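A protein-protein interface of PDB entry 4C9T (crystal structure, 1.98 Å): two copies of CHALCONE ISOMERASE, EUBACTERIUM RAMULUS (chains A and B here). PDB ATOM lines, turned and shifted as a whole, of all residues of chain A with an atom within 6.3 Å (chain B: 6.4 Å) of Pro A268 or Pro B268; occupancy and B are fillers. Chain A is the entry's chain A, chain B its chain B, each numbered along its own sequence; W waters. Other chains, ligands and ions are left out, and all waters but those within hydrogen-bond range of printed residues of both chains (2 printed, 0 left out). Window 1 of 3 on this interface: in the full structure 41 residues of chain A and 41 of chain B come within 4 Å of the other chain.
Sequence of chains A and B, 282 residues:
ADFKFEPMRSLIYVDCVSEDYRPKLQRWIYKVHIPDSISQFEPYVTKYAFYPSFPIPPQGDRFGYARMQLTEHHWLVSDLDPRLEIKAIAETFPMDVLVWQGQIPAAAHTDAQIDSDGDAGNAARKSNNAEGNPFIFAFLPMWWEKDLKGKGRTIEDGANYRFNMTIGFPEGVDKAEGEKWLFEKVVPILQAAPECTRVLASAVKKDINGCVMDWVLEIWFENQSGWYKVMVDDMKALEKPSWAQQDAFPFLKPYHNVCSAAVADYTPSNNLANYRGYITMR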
ATOM      1  N   TYR A  30     -32.829  -8.912  29.837  1.00  0.00           N
ATOM      2  CA  TYR A  30     -32.130  -8.000  30.737  1.00  0.00           C
ATOM      3  C   TYR A  30     -32.198  -8.332  32.220  1.00  0.00           C
ATOM      4  O   TYR A  30     -31.245  -8.032  32.958  1.00  0.00           O
ATOM      5  CB  TYR A  30     -32.465  -6.519  30.458  1.00  0.00           C
ATOM      6  CG  TYR A  30     -31.902  -6.012  29.183  1.00  0.00           C
ATOM      7  CD1 TYR A  30     -32.598  -6.113  28.004  1.00  0.00           C
ATOM      8  CD2 TYR A  30     -30.639  -5.417  29.130  1.00  0.00           C
ATOM      9  CE1 TYR A  30     -32.058  -5.671  26.780  1.00  0.00           C
ATOM     10  CE2 TYR A  30     -30.123  -4.980  27.936  1.00  0.00           C
ATOM     11  CZ  TYR A  30     -30.839  -5.079  26.783  1.00  0.00           C
ATOM     12  OH  TYR A  30     -30.313  -4.653  25.585  1.00  0.00           O
ATOM     13  N   PHE A  50     -24.925  -6.637  23.883  1.00  0.00           N
ATOM     14  CA  PHE A  50     -26.134  -6.681  23.063  1.00  0.00           C
ATOM     15  C   PHE A  50     -26.190  -5.369  22.295  1.00  0.00           C
ATOM     16  O   PHE A  50     -25.913  -4.269  22.856  1.00  0.00           O
ATOM     17  CB  PHE A  50     -27.385  -6.682  23.920  1.00  0.00           C
ATOM     18  CG  PHE A  50     -27.483  -7.800  24.922  1.00  0.00           C
ATOM     19  CD1 PHE A  50     -26.914  -9.045  24.716  1.00  0.00           C
ATOM     20  CD2 PHE A  50     -28.239  -7.603  26.050  1.00  0.00           C
ATOM     21  CE1 PHE A  50     -27.085 -10.085  25.624  1.00  0.00           C
ATOM     22  CE2 PHE A  50     -28.401  -8.655  27.003  1.00  0.00           C
ATOM     23  CZ  PHE A  50     -27.811  -9.856  26.792  1.00  0.00           C
ATOM     24  N   PRO A  52     -28.901  -3.502  20.227  1.00  0.00           N
ATOM     25  CA  PRO A  52     -30.318  -3.444  19.829  1.00  0.00           C
ATOM     26  C   PRO A  52     -30.437  -3.056  18.377  1.00  0.00           C
ATOM     27  O   PRO A  52     -29.737  -2.140  17.862  1.00  0.00           O
ATOM     28  CB  PRO A  52     -30.930  -2.356  20.721  1.00  0.00           C
ATOM     29  CG  PRO A  52     -29.867  -1.988  21.713  1.00  0.00           C
ATOM     30  CD  PRO A  52     -28.542  -2.492  21.241  1.00  0.00           C
ATOM     31  N   TYR A 266     -22.341   2.092  18.837  1.00  0.00           N
ATOM     32  CA  TYR A 266     -22.204   2.064  20.276  1.00  0.00           C
ATOM     33  C   TYR A 266     -23.422   1.371  20.891  1.00  0.00           C
ATOM     34  O   TYR A 266     -24.524   1.602  20.439  1.00  0.00           O
ATOM     35  CB  TYR A 266     -22.186   3.489  20.802  1.00  0.00           C
ATOM     36  CG  TYR A 266     -22.269   3.561  22.315  1.00  0.00           C
ATOM     37  CD1 TYR A 266     -21.154   3.297  23.104  1.00  0.00           C
ATOM     38  CD2 TYR A 266     -23.457   3.839  22.949  1.00  0.00           C
ATOM     39  CE1 TYR A 266     -21.228   3.343  24.491  1.00  0.00           C
ATOM     40  CE2 TYR A 266     -23.536   3.933  24.312  1.00  0.00           C
ATOM     41  CZ  TYR A 266     -22.419   3.676  25.089  1.00  0.00           C
ATOM     42  OH  TYR A 266     -22.518   3.753  26.451  1.00  0.00           O
ATOM     43  N   THR A 267     -23.227   0.572  21.919  1.00  0.00           N
ATOM     44  CA  THR A 267     -24.321   0.097  22.738  1.00  0.00           C
ATOM     45  C   THR A 267     -24.031   0.410  24.196  1.00  0.00           C
ATOM     46  O   THR A 267     -22.897   0.296  24.665  1.00  0.00           O
ATOM     47  CB  THR A 267     -24.596  -1.409  22.606  1.00  0.00           C
ATOM     48  OG1 THR A 267     -25.667  -1.766  23.523  1.00  0.00           O
ATOM     49  CG2 THR A 267     -23.334  -2.228  22.966  1.00  0.00           C
ATOM     50  N   PRO A 268     -25.060   0.808  24.956  1.00  0.00           N
ATOM     51  CA  PRO A 268     -24.867   0.877  26.386  1.00  0.00           C
ATOM     52  C   PRO A 268     -24.846  -0.494  27.045  1.00  0.00           C
ATOM     53  O   PRO A 268     -24.425  -0.572  28.198  1.00  0.00           O
ATOM     54  CB  PRO A 268     -26.084   1.620  26.887  1.00  0.00           C
ATOM     55  CG  PRO A 268     -27.128   1.379  25.860  1.00  0.00           C
ATOM     56  CD  PRO A 268     -26.405   1.212  24.537  1.00  0.00           C
ATOM     57  N   SER A 269     -25.194  -1.573  26.345  1.00  0.00           N
ATOM     58  CA  SER A 269     -25.224  -2.887  26.997  1.00  0.00           C
ATOM     59  C   SER A 269     -23.946  -3.680  26.741  1.00  0.00           C
ATOM     60  O   SER A 269     -23.928  -4.684  26.003  1.00  0.00           O
ATOM     61  CB  SER A 269     -26.423  -3.658  26.468  1.00  0.00           C
ATOM     62  OG  SER A 269     -27.575  -2.959  26.842  1.00  0.00           O
ATOM     63  N   ASN A 270     -22.874  -3.192  27.348  1.00  0.00           N
ATOM     64  CA  ASN A 270     -21.606  -3.889  27.358  1.00  0.00           C
ATOM     65  C   ASN A 270     -21.591  -4.583  28.732  1.00  0.00           C
ATOM     66  O   ASN A 270     -21.195  -4.002  29.755  1.00  0.00           O
ATOM     67  CB  ASN A 270     -20.454  -2.951  27.204  1.00  0.00           C
ATOM     68  CG  ASN A 270     -19.160  -3.699  26.980  1.00  0.00           C
ATOM     69  OD1 ASN A 270     -19.160  -4.773  26.380  1.00  0.00           O
ATOM     70  ND2 ASN A 270     -18.038  -3.077  27.330  1.00  0.00           N
ATOM     71  N   ASN A 271     -22.134  -5.768  28.747  1.00  0.00           N
ATOM     72  CA  ASN A 271     -22.705  -6.314  29.940  1.00  0.00           C
ATOM     73  C   ASN A 271     -21.679  -6.719  30.993  1.00  0.00           C
ATOM     74  O   ASN A 271     -21.961  -6.592  32.197  1.00  0.00           O
ATOM     75  CB  ASN A 271     -23.545  -7.557  29.588  1.00  0.00           C
ATOM     76  CG  ASN A 271     -24.696  -7.230  28.686  1.00  0.00           C
ATOM     77  OD1 ASN A 271     -25.324  -6.198  28.858  1.00  0.00           O
ATOM     78  ND2 ASN A 271     -25.044  -8.137  27.772  1.00  0.00           N
ATOM     79  N   ASN A 274     -20.883  -3.086  32.470  1.00  0.00           N
ATOM     80  CA  ASN A 274     -21.872  -2.014  32.709  1.00  0.00           C
ATOM     81  C   ASN A 274     -23.143  -2.475  33.455  1.00  0.00           C
ATOM     82  O   ASN A 274     -23.886  -1.610  33.901  1.00  0.00           O
ATOM     83  CB  ASN A 274     -22.407  -1.355  31.357  1.00  0.00           C
ATOM     84  CG  ASN A 274     -21.290  -0.655  30.506  1.00  0.00           C
ATOM     85  OD1 ASN A 274     -20.110  -0.557  30.887  1.00  0.00           O
ATOM     86  ND2 ASN A 274     -21.681  -0.169  29.349  1.00  0.00           N
ATOM     87  N   TYR B  30     -25.201   9.978  22.804  1.00  0.00           N
ATOM     88  CA  TYR B  30     -24.344   9.086  23.578  1.00  0.00           C
ATOM     89  C   TYR B  30     -22.882   9.425  23.525  1.00  0.00           C
ATOM     90  O   TYR B  30     -22.165   9.075  24.436  1.00  0.00           O
ATOM     91  CB  TYR B  30     -24.582   7.615  23.099  1.00  0.00           C
ATOM     92  CG  TYR B  30     -25.883   7.092  23.644  1.00  0.00           C
ATOM     93  CD1 TYR B  30     -25.954   6.499  24.925  1.00  0.00           C
ATOM     94  CD2 TYR B  30     -27.026   7.164  22.901  1.00  0.00           C
ATOM     95  CE1 TYR B  30     -27.165   6.012  25.420  1.00  0.00           C
ATOM     96  CE2 TYR B  30     -28.227   6.711  23.403  1.00  0.00           C
ATOM     97  CZ  TYR B  30     -28.280   6.134  24.678  1.00  0.00           C
ATOM     98  OH  TYR B  30     -29.488   5.665  25.134  1.00  0.00           O
ATOM     99  N   PHE B  50     -31.628   7.724  30.276  1.00  0.00           N
ATOM    100  CA  PHE B  50     -32.342   7.743  29.063  1.00  0.00           C
ATOM    101  C   PHE B  50     -33.158   6.451  28.997  1.00  0.00           C
ATOM    102  O   PHE B  50     -32.623   5.380  29.235  1.00  0.00           O
ATOM    103  CB  PHE B  50     -31.441   7.766  27.822  1.00  0.00           C
ATOM    104  CG  PHE B  50     -30.424   8.857  27.777  1.00  0.00           C
ATOM    105  CD1 PHE B  50     -30.663  10.116  28.280  1.00  0.00           C
ATOM    106  CD2 PHE B  50     -29.223   8.638  27.097  1.00  0.00           C
ATOM    107  CE1 PHE B  50     -29.707  11.095  28.196  1.00  0.00           C
ATOM    108  CE2 PHE B  50     -28.278   9.632  26.980  1.00  0.00           C
ATOM    109  CZ  PHE B  50     -28.517  10.855  27.510  1.00  0.00           C
ATOM    110  N   PRO B  52     -35.054   4.567  26.102  1.00  0.00           N
ATOM    111  CA  PRO B  52     -35.372   4.564  24.657  1.00  0.00           C
ATOM    112  C   PRO B  52     -36.826   4.176  24.481  1.00  0.00           C
ATOM    113  O   PRO B  52     -37.348   3.302  25.242  1.00  0.00           O
ATOM    114  CB  PRO B  52     -34.512   3.494  24.090  1.00  0.00           C
ATOM    115  CG  PRO B  52     -33.695   2.951  25.198  1.00  0.00           C
ATOM    116  CD  PRO B  52     -34.046   3.593  26.474  1.00  0.00           C
ATOM    117  N   TYR B 266     -36.834  -1.129  32.578  1.00  0.00           N
ATOM    118  CA  TYR B 266     -35.416  -1.009  32.778  1.00  0.00           C
ATOM    119  C   TYR B 266     -34.768  -0.306  31.592  1.00  0.00           C
ATOM    120  O   TYR B 266     -35.152  -0.514  30.448  1.00  0.00           O
ATOM    121  CB  TYR B 266     -34.832  -2.424  32.896  1.00  0.00           C
ATOM    122  CG  TYR B 266     -33.303  -2.498  32.822  1.00  0.00           C
ATOM    123  CD1 TYR B 266     -32.542  -2.254  33.931  1.00  0.00           C
ATOM    124  CD2 TYR B 266     -32.646  -2.824  31.637  1.00  0.00           C
ATOM    125  CE1 TYR B 266     -31.141  -2.310  33.889  1.00  0.00           C
ATOM    126  CE2 TYR B 266     -31.250  -2.907  31.557  1.00  0.00           C
ATOM    127  CZ  TYR B 266     -30.521  -2.644  32.702  1.00  0.00           C
ATOM    128  OH  TYR B 266     -29.173  -2.678  32.700  1.00  0.00           O
ATOM    129  N   THR B 267     -33.730   0.451  31.871  1.00  0.00           N
ATOM    130  CA  THR B 267     -32.805   0.931  30.880  1.00  0.00           C
ATOM    131  C   THR B 267     -31.360   0.637  31.217  1.00  0.00           C
ATOM    132  O   THR B 267     -30.951   0.785  32.354  1.00  0.00           O
ATOM    133  CB  THR B 267     -32.918   2.449  30.635  1.00  0.00           C
ATOM    134  OG1 THR B 267     -32.033   2.809  29.575  1.00  0.00           O
ATOM    135  CG2 THR B 267     -32.552   3.297  31.834  1.00  0.00           C
ATOM    136  N   PRO B 268     -30.547   0.302  30.212  1.00  0.00           N
ATOM    137  CA  PRO B 268     -29.113   0.170  30.435  1.00  0.00           C
ATOM    138  C   PRO B 268     -28.457   1.545  30.497  1.00  0.00           C
ATOM    139  O   PRO B 268     -27.356   1.630  31.004  1.00  0.00           O
ATOM    140  CB  PRO B 268     -28.591  -0.620  29.243  1.00  0.00           C
ATOM    141  CG  PRO B 268     -29.599  -0.356  28.170  1.00  0.00           C
ATOM    142  CD  PRO B 268     -30.966  -0.146  28.874  1.00  0.00           C
ATOM    143  N   SER B 269     -29.169   2.611  30.116  1.00  0.00           N
ATOM    144  CA  SER B 269     -28.537   3.938  30.058  1.00  0.00           C
ATOM    145  C   SER B 269     -28.820   4.715  31.342  1.00  0.00           C
ATOM    146  O   SER B 269     -29.529   5.708  31.355  1.00  0.00           O
ATOM    147  CB  SER B 269     -28.985   4.681  28.818  1.00  0.00           C
ATOM    148  OG  SER B 269     -28.585   3.940  27.694  1.00  0.00           O
ATOM    149  N   ASN B 270     -28.268   4.222  32.427  1.00  0.00           N
ATOM    150  CA  ASN B 270     -28.281   4.947  33.725  1.00  0.00           C
ATOM    151  C   ASN B 270     -26.911   5.617  33.820  1.00  0.00           C
ATOM    152  O   ASN B 270     -25.954   5.009  34.276  1.00  0.00           O
ATOM    153  CB  ASN B 270     -28.473   4.003  34.917  1.00  0.00           C
ATOM    154  CG  ASN B 270     -28.807   4.754  36.176  1.00  0.00           C
ATOM    155  OD1 ASN B 270     -29.361   5.826  36.122  1.00  0.00           O
ATOM    156  ND2 ASN B 270     -28.471   4.190  37.322  1.00  0.00           N
ATOM    157  N   ASN B 271     -26.847   6.831  33.307  1.00  0.00           N
ATOM    158  CA  ASN B 271     -25.618   7.403  32.807  1.00  0.00           C
ATOM    159  C   ASN B 271     -24.596   7.751  33.858  1.00  0.00           C
ATOM    160  O   ASN B 271     -23.394   7.596  33.584  1.00  0.00           O
ATOM    161  CB  ASN B 271     -25.920   8.616  31.917  1.00  0.00           C
ATOM    162  CG  ASN B 271     -26.791   8.279  30.786  1.00  0.00           C
ATOM    163  OD1 ASN B 271     -26.634   7.239  30.205  1.00  0.00           O
ATOM    164  ND2 ASN B 271     -27.688   9.179  30.421  1.00  0.00           N
ATOM    165  N   ASN B 274     -23.216   4.101  34.641  1.00  0.00           N
ATOM    166  CA  ASN B 274     -22.999   3.068  33.643  1.00  0.00           C
ATOM    167  C   ASN B 274     -22.164   3.494  32.443  1.00  0.00           C
ATOM    168  O   ASN B 274     -21.724   2.633  31.676  1.00  0.00           O
ATOM    169  CB  ASN B 274     -24.368   2.544  33.071  1.00  0.00           C
ATOM    170  CG  ASN B 274     -25.189   1.713  34.124  1.00  0.00           C
ATOM    171  OD1 ASN B 274     -24.855   1.597  35.327  1.00  0.00           O
ATOM    172  ND2 ASN B 274     -26.276   1.176  33.669  1.00  0.00           N
HETATM  173  O   HOH W   1     -21.784  -0.011  35.665  1.00  0.00           O
HETATM  174  O   HOH W   2     -19.999   0.946  33.661  1.00  0.00           O
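The backbone NH (N) of Phe A50 lies within hydrogen-bond range of the backbone carbonyl oxygen (O) of Ser A269. The side-chain amide nitrogen (ND2) of Asn A274 is in hydrogen-bond range of the backbone carbonyl oxygen (O) of Pro A268 (3.0 Å). The side-chain hydroxyl (OG) of Ser B269 lies within hydrogen-bond range of the side-chain hydroxyl (OH) of Tyr B30, 3.2 Å away. O of Ser B269 is in hydrogen-bond range of N of Phe B50 (3.1 Å). The backbone NH (N) of Ser B269 is in hydrogen-bond range of the side-chain hydroxyl (OG1) of Thr B267. The side-chain amide nitrogen (ND2) of Asn B274 lies within hydrogen-bond range of the backbone carbonyl oxygen (O) of Pro B268.
Among the printed residues, merely in contact across the chains: Tyr A30 with Tyr B266, Tyr A266 with Tyr B30, Pro A268 with Pro B268, Pro A268 with Ser B269, Ser A269 with Pro B268 and Asn A274 with Asn B274.
Printed residues of chain B within 4 Å of Pro A268: Pro B268 and Ser B269. Of the printed residues of chain A, Ser B269 touches Pro A268. Of the printed residues of chain B, Asn A274 touches Asn B274 (3.5 Å). Printed residues of chain B within 4 Å of Tyr A30: Tyr B266 (3.5 Å). Of the printed residues of chain A, Tyr B266 touches Tyr A30 (3.5 Å). Pro B52 touches none of the printed residues of chain A. Pro A52 touches none of the printed residues of chain B.
Of the 10 printed residues of chain A, 5 touch a printed residue of chain B. Along chain A the printed residues that touch a printed residue of chain B span positions 30 to 274. Along chain B the printed residues that touch a printed residue of chain A span positions 30 to 274. Among the printed residues, 6 pairs touch across the chains.
Tyr A30 touches Tyr B266, and with the chains exchanged Tyr A266 touches Tyr B30. Pro B268 touches its own counterpart, Pro A268. Pro A268 touches Ser B269, and with the chains exchanged Ser A269 touches Pro B268. Asn B274 touches its own counterpart, Asn A274. Positions printed for both chains: 30, 50, 52, 266, 267, 268, 269, 270, 271 and 274. Of the 6 pairs that touch across the chains among the printed residues, 6 have their exchanged pair printed and touching as well.
Water W2 bridges O of Asn B274 and OD1 of Asn A274. Water W1 bridges O of Asn A274 (3.2 Å) and OD1 of Asn B274 (3.5 Å).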
